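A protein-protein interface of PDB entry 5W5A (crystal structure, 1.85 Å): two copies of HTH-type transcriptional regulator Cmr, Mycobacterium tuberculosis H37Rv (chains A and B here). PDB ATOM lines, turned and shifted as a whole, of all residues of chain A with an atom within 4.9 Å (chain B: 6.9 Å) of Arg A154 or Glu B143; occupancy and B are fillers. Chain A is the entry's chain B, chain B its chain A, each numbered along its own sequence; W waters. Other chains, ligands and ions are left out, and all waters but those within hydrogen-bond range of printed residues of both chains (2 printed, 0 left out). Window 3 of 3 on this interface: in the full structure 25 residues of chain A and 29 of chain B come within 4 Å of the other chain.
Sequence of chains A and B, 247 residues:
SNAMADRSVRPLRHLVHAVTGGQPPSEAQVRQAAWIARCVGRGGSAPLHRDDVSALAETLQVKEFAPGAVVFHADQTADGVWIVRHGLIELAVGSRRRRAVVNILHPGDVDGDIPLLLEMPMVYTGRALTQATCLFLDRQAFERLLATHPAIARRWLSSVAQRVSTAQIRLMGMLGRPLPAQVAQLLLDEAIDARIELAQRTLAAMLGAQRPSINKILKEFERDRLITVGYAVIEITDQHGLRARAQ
Water W1 lies within hydrogen-bond range of the side-chain hydroxyl (OG) of Ser A158, the backbone carbonyl oxygen (O) of Leu B117 and the guanidinium group (NH2) of Arg A154.
Water W2 lies within hydrogen-bond range of the backbone carbonyl oxygen of Pro A150 (2.5 Å) and the backbone carbonyl oxygen of Leu B146 (2.9 Å).
Of the 17 printed residues of chain B, 4 touch a printed residue of chain A.
Hydrophobic or aromatic side chains of chain B that line the printed part of chain A: Leu B117 and Leu B146.
Along chain B the printed residues that touch a printed residue of chain A span positions 117 to 147.
Among the printed residues, Asp or Glu carboxylates within 4 Å of a Lys or Arg side-chain nitrogen of the other chain: Arg A154 with Glu B143 (2.8 Å).
The side-chain hydroxyl of Ser A158 sits at hydrogen-bond distance from the guanidinium group of Arg A154, 2.8 Å away.
Position printed for both chains: 153.
Among the printed residues, merely in contact across the chains: Pro A150 with Ala B147 (3.6 Å), Arg A154 with Leu B117 (3.4 Å), Arg A154 with Leu B146 (3.7 Å), Leu A157 with Leu B117 (3.8 Å) and Leu A157 with Leu B146 (3.8 Å).
Printed residues of chain B within 4 Å of Pro A150: Ala B147 (3.6 Å).
Arg A154 touches just these residues of chain B: Leu B117, Glu B143 and Leu B146.
Of the printed residues of chain B, Leu A157 touches Leu B117 and Leu B146.
Leu B116 touches none of the printed residues of chain A.
Of the printed residues of chain A, Leu B117 touches Arg A154 (3.4 Å) and Leu A157 (3.8 Å).
Glu B143 touches one residue of chain A.
Printed residues of chain A within 4 Å of Ala B147: Pro A150.
Thr B148 touches none of the printed residues of chain A.
The nearest residue of chain B that does not touch Arg A154 is Phe B142 (4.5 Å).
The nearest printed residue of chain A that does not touch Glu B143 is Ser A158 (6.9 Å).
The nearest printed residue of chain A that does not touch Ala B147 is Arg A154 (6.3 Å).
OE1 of Glu B143 is in salt-bridge range of NE of Arg A154 (2.8 Å).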
ATOM      1  N   PRO A 150       1.360   4.762  17.272  1.00  0.00           N
ATOM      2  CA  PRO A 150       0.543   5.065  16.098  1.00  0.00           C
ATOM      3  C   PRO A 150       1.230   5.973  15.111  1.00  0.00           C
ATOM      4  O   PRO A 150       1.099   5.740  13.893  1.00  0.00           O
ATOM      5  CB  PRO A 150      -0.691   5.744  16.702  1.00  0.00           C
ATOM      6  CG  PRO A 150      -0.821   5.092  18.081  1.00  0.00           C
ATOM      7  CD  PRO A 150       0.618   4.963  18.544  1.00  0.00           C
ATOM      8  N   ALA A 151       1.968   6.971  15.602  1.00  0.00           N
ATOM      9  CA  ALA A 151       2.605   7.911  14.688  1.00  0.00           C
ATOM     10  C   ALA A 151       3.718   7.221  13.919  1.00  0.00           C
ATOM     11  O   ALA A 151       3.963   7.511  12.741  1.00  0.00           O
ATOM     12  CB  ALA A 151       3.142   9.157  15.456  1.00  0.00           C
ATOM     13  N   ILE A 152       4.418   6.311  14.585  1.00  0.00           N
ATOM     14  CA  ILE A 152       5.449   5.537  13.903  1.00  0.00           C
ATOM     15  C   ILE A 152       4.838   4.577  12.875  1.00  0.00           C
ATOM     16  O   ILE A 152       5.310   4.482  11.748  1.00  0.00           O
ATOM     17  CB  ILE A 152       6.314   4.783  14.920  1.00  0.00           C
ATOM     18  CG1 ILE A 152       7.208   5.805  15.638  1.00  0.00           C
ATOM     19  CG2 ILE A 152       7.122   3.696  14.229  1.00  0.00           C
ATOM     20  CD1 ILE A 152       8.055   5.212  16.748  1.00  0.00           C
ATOM     21  N   ALA A 153       3.742   3.917  13.224  1.00  0.00           N
ATOM     22  CA  ALA A 153       3.051   3.059  12.269  1.00  0.00           C
ATOM     23  C   ALA A 153       2.606   3.840  11.035  1.00  0.00           C
ATOM     24  O   ALA A 153       2.695   3.358   9.900  1.00  0.00           O
ATOM     25  CB  ALA A 153       1.847   2.389  12.946  1.00  0.00           C
ATOM     26  N   ARG A 154       2.141   5.063  11.257  1.00  0.00           N
ATOM     27  CA  ARG A 154       1.605   5.875  10.183  1.00  0.00           C
ATOM     28  C   ARG A 154       2.722   6.314   9.213  1.00  0.00           C
ATOM     29  O   ARG A 154       2.526   6.330   8.003  1.00  0.00           O
ATOM     30  CB  ARG A 154       0.881   7.102  10.760  1.00  0.00           C
ATOM     31  CG  ARG A 154       0.324   8.084   9.722  1.00  0.00           C
ATOM     32  CD  ARG A 154      -0.777   7.409   8.841  1.00  0.00           C
ATOM     33  NE  ARG A 154      -1.299   8.327   7.820  1.00  0.00           N
ATOM     34  CZ  ARG A 154      -0.702   8.538   6.658  1.00  0.00           C
ATOM     35  NH1 ARG A 154       0.438   7.902   6.373  1.00  0.00           N
ATOM     36  NH2 ARG A 154      -1.222   9.376   5.792  1.00  0.00           N
ATOM     37  N   ARG A 155       3.871   6.715   9.752  1.00  0.00           N
ATOM     38  CA  ARG A 155       4.959   7.140   8.878  1.00  0.00           C
ATOM     39  C   ARG A 155       5.541   5.951   8.139  1.00  0.00           C
ATOM     40  O   ARG A 155       5.916   6.057   6.949  1.00  0.00           O
ATOM     41  CB  ARG A 155       6.059   7.867   9.675  1.00  0.00           C
ATOM     42  CG  ARG A 155       7.333   8.106   8.864  1.00  0.00           C
ATOM     43  CD  ARG A 155       8.399   8.893   9.672  1.00  0.00           C
ATOM     44  NE  ARG A 155       9.568   9.124   8.833  1.00  0.00           N
ATOM     45  CZ  ARG A 155      10.223  10.272   8.725  1.00  0.00           C
ATOM     46  NH1 ARG A 155       9.853  11.345   9.409  1.00  0.00           N
ATOM     47  NH2 ARG A 155      11.262  10.333   7.911  1.00  0.00           N
ATOM     48  N   TRP A 156       5.590   4.800   8.810  1.00  0.00           N
ATOM     49  CA  TRP A 156       6.017   3.573   8.129  1.00  0.00           C
ATOM     50  C   TRP A 156       5.130   3.255   6.934  1.00  0.00           C
ATOM     51  O   TRP A 156       5.604   2.821   5.858  1.00  0.00           O
ATOM     52  CB  TRP A 156       6.058   2.355   9.088  1.00  0.00           C
ATOM     53  CG  TRP A 156       7.321   1.527   8.818  1.00  0.00           C
ATOM     54  CD1 TRP A 156       7.676   0.915   7.642  1.00  0.00           C
ATOM     55  CD2 TRP A 156       8.408   1.313   9.726  1.00  0.00           C
ATOM     56  NE1 TRP A 156       8.929   0.319   7.779  1.00  0.00           N
ATOM     57  CE2 TRP A 156       9.386   0.548   9.050  1.00  0.00           C
ATOM     58  CE3 TRP A 156       8.649   1.688  11.053  1.00  0.00           C
ATOM     59  CZ2 TRP A 156      10.589   0.157   9.660  1.00  0.00           C
ATOM     60  CZ3 TRP A 156       9.844   1.284  11.663  1.00  0.00           C
ATOM     61  CH2 TRP A 156      10.794   0.529  10.957  1.00  0.00           C
ATOM     62  N   LEU A 157       3.831   3.441   7.105  1.00  0.00           N
ATOM     63  CA  LEU A 157       2.901   3.190   6.001  1.00  0.00           C
ATOM     64  C   LEU A 157       3.163   4.128   4.786  1.00  0.00           C
ATOM     65  O   LEU A 157       3.145   3.680   3.633  1.00  0.00           O
ATOM     66  CB  LEU A 157       1.442   3.329   6.512  1.00  0.00           C
ATOM     67  CG  LEU A 157       0.281   3.158   5.525  1.00  0.00           C
ATOM     68  CD1 LEU A 157       0.290   1.791   4.763  1.00  0.00           C
ATOM     69  CD2 LEU A 157      -1.071   3.336   6.286  1.00  0.00           C
ATOM     70  N   SER A 158       3.393   5.415   5.058  1.00  0.00           N
ATOM     71  CA  SER A 158       3.768   6.409   4.039  1.00  0.00           C
ATOM     72  C   SER A 158       5.049   6.014   3.323  1.00  0.00           C
ATOM     73  O   SER A 158       5.164   6.116   2.101  1.00  0.00           O
ATOM     74  CB  SER A 158       3.986   7.796   4.672  1.00  0.00           C
ATOM     75  OG  SER A 158       2.730   8.447   4.829  1.00  0.00           O
ATOM     76  N   LEU B 116      -4.096   8.376  -1.984  1.00  0.00           N
ATOM     77  CA  LEU B 116      -4.292   9.203  -0.797  1.00  0.00           C
ATOM     78  C   LEU B 116      -3.026   9.268   0.069  1.00  0.00           C
ATOM     79  O   LEU B 116      -2.591  10.346   0.495  1.00  0.00           O
ATOM     80  CB  LEU B 116      -5.452   8.662   0.010  1.00  0.00           C
ATOM     81  CG  LEU B 116      -5.833   9.361   1.307  1.00  0.00           C
ATOM     82  CD1 LEU B 116      -6.470  10.699   1.006  1.00  0.00           C
ATOM     83  CD2 LEU B 116      -6.813   8.456   2.063  1.00  0.00           C
ATOM     84  N   LEU B 117      -2.434   8.108   0.330  1.00  0.00           N
ATOM     85  CA  LEU B 117      -1.179   8.047   1.091  1.00  0.00           C
ATOM     86  C   LEU B 117      -0.052   8.833   0.403  1.00  0.00           C
ATOM     87  O   LEU B 117       0.771   9.453   1.077  1.00  0.00           O
ATOM     88  CB  LEU B 117      -0.758   6.580   1.298  1.00  0.00           C
ATOM     89  CG  LEU B 117      -1.554   5.826   2.371  1.00  0.00           C
ATOM     90  CD1 LEU B 117      -1.290   4.360   2.260  1.00  0.00           C
ATOM     91  CD2 LEU B 117      -1.118   6.334   3.736  1.00  0.00           C
ATOM     92  N   LEU B 118      -0.035   8.830  -0.931  1.00  0.00           N
ATOM     93  CA  LEU B 118       1.021   9.492  -1.700  1.00  0.00           C
ATOM     94  C   LEU B 118       0.709  10.962  -2.008  1.00  0.00           C
ATOM     95  O   LEU B 118       1.541  11.693  -2.571  1.00  0.00           O
ATOM     96  CB  LEU B 118       1.269   8.734  -3.013  1.00  0.00           C
ATOM     97  CG  LEU B 118       1.770   7.283  -2.972  1.00  0.00           C
ATOM     98  CD1 LEU B 118       1.694   6.629  -4.360  1.00  0.00           C
ATOM     99  CD2 LEU B 118       3.172   7.233  -2.435  1.00  0.00           C
ATOM    100  N   GLU B 119      -0.490  11.390  -1.633  1.00  0.00           N
ATOM    101  CA  GLU B 119      -1.005  12.723  -1.968  1.00  0.00           C
ATOM    102  C   GLU B 119      -1.023  12.939  -3.470  1.00  0.00           C
ATOM    103  O   GLU B 119      -0.624  13.991  -3.964  1.00  0.00           O
ATOM    104  CB  GLU B 119      -0.184  13.834  -1.296  1.00  0.00           C
ATOM    105  CG  GLU B 119       0.079  13.628   0.178  1.00  0.00           C
ATOM    106  CD  GLU B 119      -0.759  14.528   1.063  1.00  0.00           C
ATOM    107  OE1 GLU B 119      -1.340  15.501   0.535  1.00  0.00           O
ATOM    108  OE2 GLU B 119      -0.837  14.263   2.287  1.00  0.00           O
ATOM    109  N   LEU B 137     -14.520   6.332   2.918  1.00  0.00           N
ATOM    110  CA  LEU B 137     -13.824   6.670   4.156  1.00  0.00           C
ATOM    111  C   LEU B 137     -13.008   7.914   3.868  1.00  0.00           C
ATOM    112  O   LEU B 137     -11.960   7.840   3.226  1.00  0.00           O
ATOM    113  CB  LEU B 137     -12.946   5.489   4.632  1.00  0.00           C
ATOM    114  CG  LEU B 137     -12.173   5.577   5.958  1.00  0.00           C
ATOM    115  CD1 LEU B 137     -13.106   5.387   7.153  1.00  0.00           C
ATOM    116  CD2 LEU B 137     -11.013   4.559   5.967  1.00  0.00           C
ATOM    117  N   ASP B 138     -13.493   9.079   4.303  1.00  0.00           N
ATOM    118  CA  ASP B 138     -12.819  10.303   3.871  1.00  0.00           C
ATOM    119  C   ASP B 138     -11.461  10.434   4.581  1.00  0.00           C
ATOM    120  O   ASP B 138     -11.147   9.646   5.481  1.00  0.00           O
ATOM    121  CB  ASP B 138     -13.724  11.537   4.062  1.00  0.00           C
ATOM    122  CG  ASP B 138     -13.993  11.913   5.525  1.00  0.00           C
ATOM    123  OD1 ASP B 138     -13.313  11.467   6.468  1.00  0.00           O
ATOM    124  OD2 ASP B 138     -14.912  12.740   5.726  1.00  0.00           O
ATOM    125  N   ARG B 139     -10.641  11.382   4.130  1.00  0.00           N
ATOM    126  CA  ARG B 139      -9.269  11.499   4.606  1.00  0.00           C
ATOM    127  C   ARG B 139      -9.204  11.609   6.121  1.00  0.00           C
ATOM    128  O   ARG B 139      -8.414  10.933   6.760  1.00  0.00           O
ATOM    129  CB  ARG B 139      -8.568  12.720   3.979  1.00  0.00           C
ATOM    130  CG  ARG B 139      -7.125  12.913   4.462  1.00  0.00           C
ATOM    131  CD  ARG B 139      -6.551  14.273   4.064  1.00  0.00           C
ATOM    132  NE  ARG B 139      -6.747  14.552   2.645  1.00  0.00           N
ATOM    133  CZ  ARG B 139      -5.951  14.125   1.670  1.00  0.00           C
ATOM    134  NH1 ARG B 139      -4.880  13.378   1.946  1.00  0.00           N
ATOM    135  NH2 ARG B 139      -6.232  14.445   0.414  1.00  0.00           N
ATOM    136  N   GLN B 140     -10.041  12.480   6.677  1.00  0.00           N
ATOM    137  CA  GLN B 140     -10.070  12.681   8.113  1.00  0.00           C
ATOM    138  C   GLN B 140     -10.412  11.386   8.872  1.00  0.00           C
ATOM    139  O   GLN B 140      -9.794  11.078   9.887  1.00  0.00           O
ATOM    140  CB  GLN B 140     -11.077  13.781   8.461  1.00  0.00           C
ATOM    141  CG  GLN B 140     -11.293  13.948   9.934  1.00  0.00           C
ATOM    142  CD  GLN B 140     -11.985  15.258  10.254  1.00  0.00           C
ATOM    143  OE1 GLN B 140     -11.734  15.861  11.295  1.00  0.00           O
ATOM    144  NE2 GLN B 140     -12.854  15.707   9.350  1.00  0.00           N
ATOM    145  N   ALA B 141     -11.387  10.629   8.374  1.00  0.00           N
ATOM    146  CA  ALA B 141     -11.775   9.374   9.026  1.00  0.00           C
ATOM    147  C   ALA B 141     -10.690   8.308   8.887  1.00  0.00           C
ATOM    148  O   ALA B 141     -10.437   7.509   9.797  1.00  0.00           O
ATOM    149  CB  ALA B 141     -13.102   8.870   8.435  1.00  0.00           C
ATOM    150  N   PHE B 142     -10.065   8.295   7.715  1.00  0.00           N
ATOM    151  CA  PHE B 142      -8.942   7.394   7.448  1.00  0.00           C
ATOM    152  C   PHE B 142      -7.805   7.633   8.445  1.00  0.00           C
ATOM    153  O   PHE B 142      -7.277   6.680   9.014  1.00  0.00           O
ATOM    154  CB  PHE B 142      -8.486   7.595   6.002  1.00  0.00           C
ATOM    155  CG  PHE B 142      -7.216   6.838   5.613  1.00  0.00           C
ATOM    156  CD1 PHE B 142      -7.216   5.462   5.519  1.00  0.00           C
ATOM    157  CD2 PHE B 142      -6.046   7.533   5.309  1.00  0.00           C
ATOM    158  CE1 PHE B 142      -6.059   4.767   5.113  1.00  0.00           C
ATOM    159  CE2 PHE B 142      -4.871   6.850   4.911  1.00  0.00           C
ATOM    160  CZ  PHE B 142      -4.892   5.469   4.808  1.00  0.00           C
ATOM    161  N   GLU B 143      -7.445   8.895   8.672  1.00  0.00           N
ATOM    162  CA  GLU B 143      -6.355   9.197   9.610  1.00  0.00           C
ATOM    163  C   GLU B 143      -6.753   8.821  11.034  1.00  0.00           C
ATOM    164  O   GLU B 143      -5.948   8.267  11.788  1.00  0.00           O
ATOM    165  CB  GLU B 143      -5.951  10.679   9.555  1.00  0.00           C
ATOM    166  CG  GLU B 143      -5.388  11.136   8.190  1.00  0.00           C
ATOM    167  CD  GLU B 143      -4.014  10.527   7.888  1.00  0.00           C
ATOM    168  OE1 GLU B 143      -3.400   9.917   8.791  1.00  0.00           O
ATOM    169  OE2 GLU B 143      -3.539  10.684   6.747  1.00  0.00           O
ATOM    170  N   ARG B 144      -8.008   9.082  11.390  1.00  0.00           N
ATOM    171  CA  ARG B 144      -8.475   8.779  12.733  1.00  0.00           C
ATOM    172  C   ARG B 144      -8.456   7.275  12.958  1.00  0.00           C
ATOM    173  O   ARG B 144      -8.062   6.802  14.035  1.00  0.00           O
ATOM    174  CB  ARG B 144      -9.892   9.344  12.964  1.00  0.00           C
ATOM    175  CG  ARG B 144     -10.413   9.171  14.377  1.00  0.00           C
ATOM    176  CD  ARG B 144     -11.614  10.085  14.608  1.00  0.00           C
ATOM    177  NE  ARG B 144     -11.266  11.500  14.437  1.00  0.00           N
ATOM    178  CZ  ARG B 144     -11.627  12.256  13.399  1.00  0.00           C
ATOM    179  NH1 ARG B 144     -12.377  11.754  12.420  1.00  0.00           N
ATOM    180  NH2 ARG B 144     -11.241  13.527  13.349  1.00  0.00           N
ATOM    181  N   LEU B 145      -8.921   6.517  11.965  1.00  0.00           N
ATOM    182  CA  LEU B 145      -8.871   5.050  12.043  1.00  0.00           C
ATOM    183  C   LEU B 145      -7.461   4.530  12.240  1.00  0.00           C
ATOM    184  O   LEU B 145      -7.209   3.698  13.124  1.00  0.00           O
ATOM    185  CB  LEU B 145      -9.452   4.419  10.772  1.00  0.00           C
ATOM    186  CG  LEU B 145      -9.537   2.889  10.763  1.00  0.00           C
ATOM    187  CD1 LEU B 145     -10.358   2.379  11.923  1.00  0.00           C
ATOM    188  CD2 LEU B 145     -10.137   2.392   9.456  1.00  0.00           C
ATOM    189  N   LEU B 146      -6.540   4.993  11.400  1.00  0.00           N
ATOM    190  CA  LEU B 146      -5.139   4.557  11.508  1.00  0.00           C
ATOM    191  C   LEU B 146      -4.499   4.936  12.855  1.00  0.00           C
ATOM    192  O   LEU B 146      -3.648   4.204  13.372  1.00  0.00           O
ATOM    193  CB  LEU B 146      -4.326   5.145  10.376  1.00  0.00           C
ATOM    194  CG  LEU B 146      -4.633   4.623   8.969  1.00  0.00           C
ATOM    195  CD1 LEU B 146      -3.746   5.385   7.982  1.00  0.00           C
ATOM    196  CD2 LEU B 146      -4.328   3.162   8.910  1.00  0.00           C
ATOM    197  N   ALA B 147      -4.930   6.068  13.402  1.00  0.00           N
ATOM    198  CA  ALA B 147      -4.416   6.561  14.682  1.00  0.00           C
ATOM    199  C   ALA B 147      -4.949   5.752  15.878  1.00  0.00           C
ATOM    200  O   ALA B 147      -4.329   5.748  16.928  1.00  0.00           O
ATOM    201  CB  ALA B 147      -4.750   8.031  14.850  1.00  0.00           C
ATOM    202  N   THR B 148      -6.054   5.032  15.710  1.00  0.00           N
ATOM    203  CA  THR B 148      -6.707   4.410  16.864  1.00  0.00           C
ATOM    204  C   THR B 148      -6.984   2.905  16.762  1.00  0.00           C
ATOM    205  O   THR B 148      -7.494   2.322  17.706  1.00  0.00           O
ATOM    206  CB  THR B 148      -8.062   5.100  17.168  1.00  0.00           C
ATOM    207  OG1 THR B 148      -8.901   5.041  16.014  1.00  0.00           O
ATOM    208  CG2 THR B 148      -7.850   6.580  17.541  1.00  0.00           C
ATOM    209  N   ALA B 153      -4.154  -0.647  11.143  1.00  0.00           N
ATOM    210  CA  ALA B 153      -2.941   0.068  10.717  1.00  0.00           C
ATOM    211  C   ALA B 153      -1.851  -0.928  10.270  1.00  0.00           C
ATOM    212  O   ALA B 153      -1.218  -0.725   9.226  1.00  0.00           O
ATOM    213  CB  ALA B 153      -2.411   0.950  11.834  1.00  0.00           C
HETATM  214  O   HOH W   1       0.884   9.734   3.877  1.00  0.00           O
HETATM  215  O   HOH W   2      -1.149   5.657  12.813  1.00  0.00           O
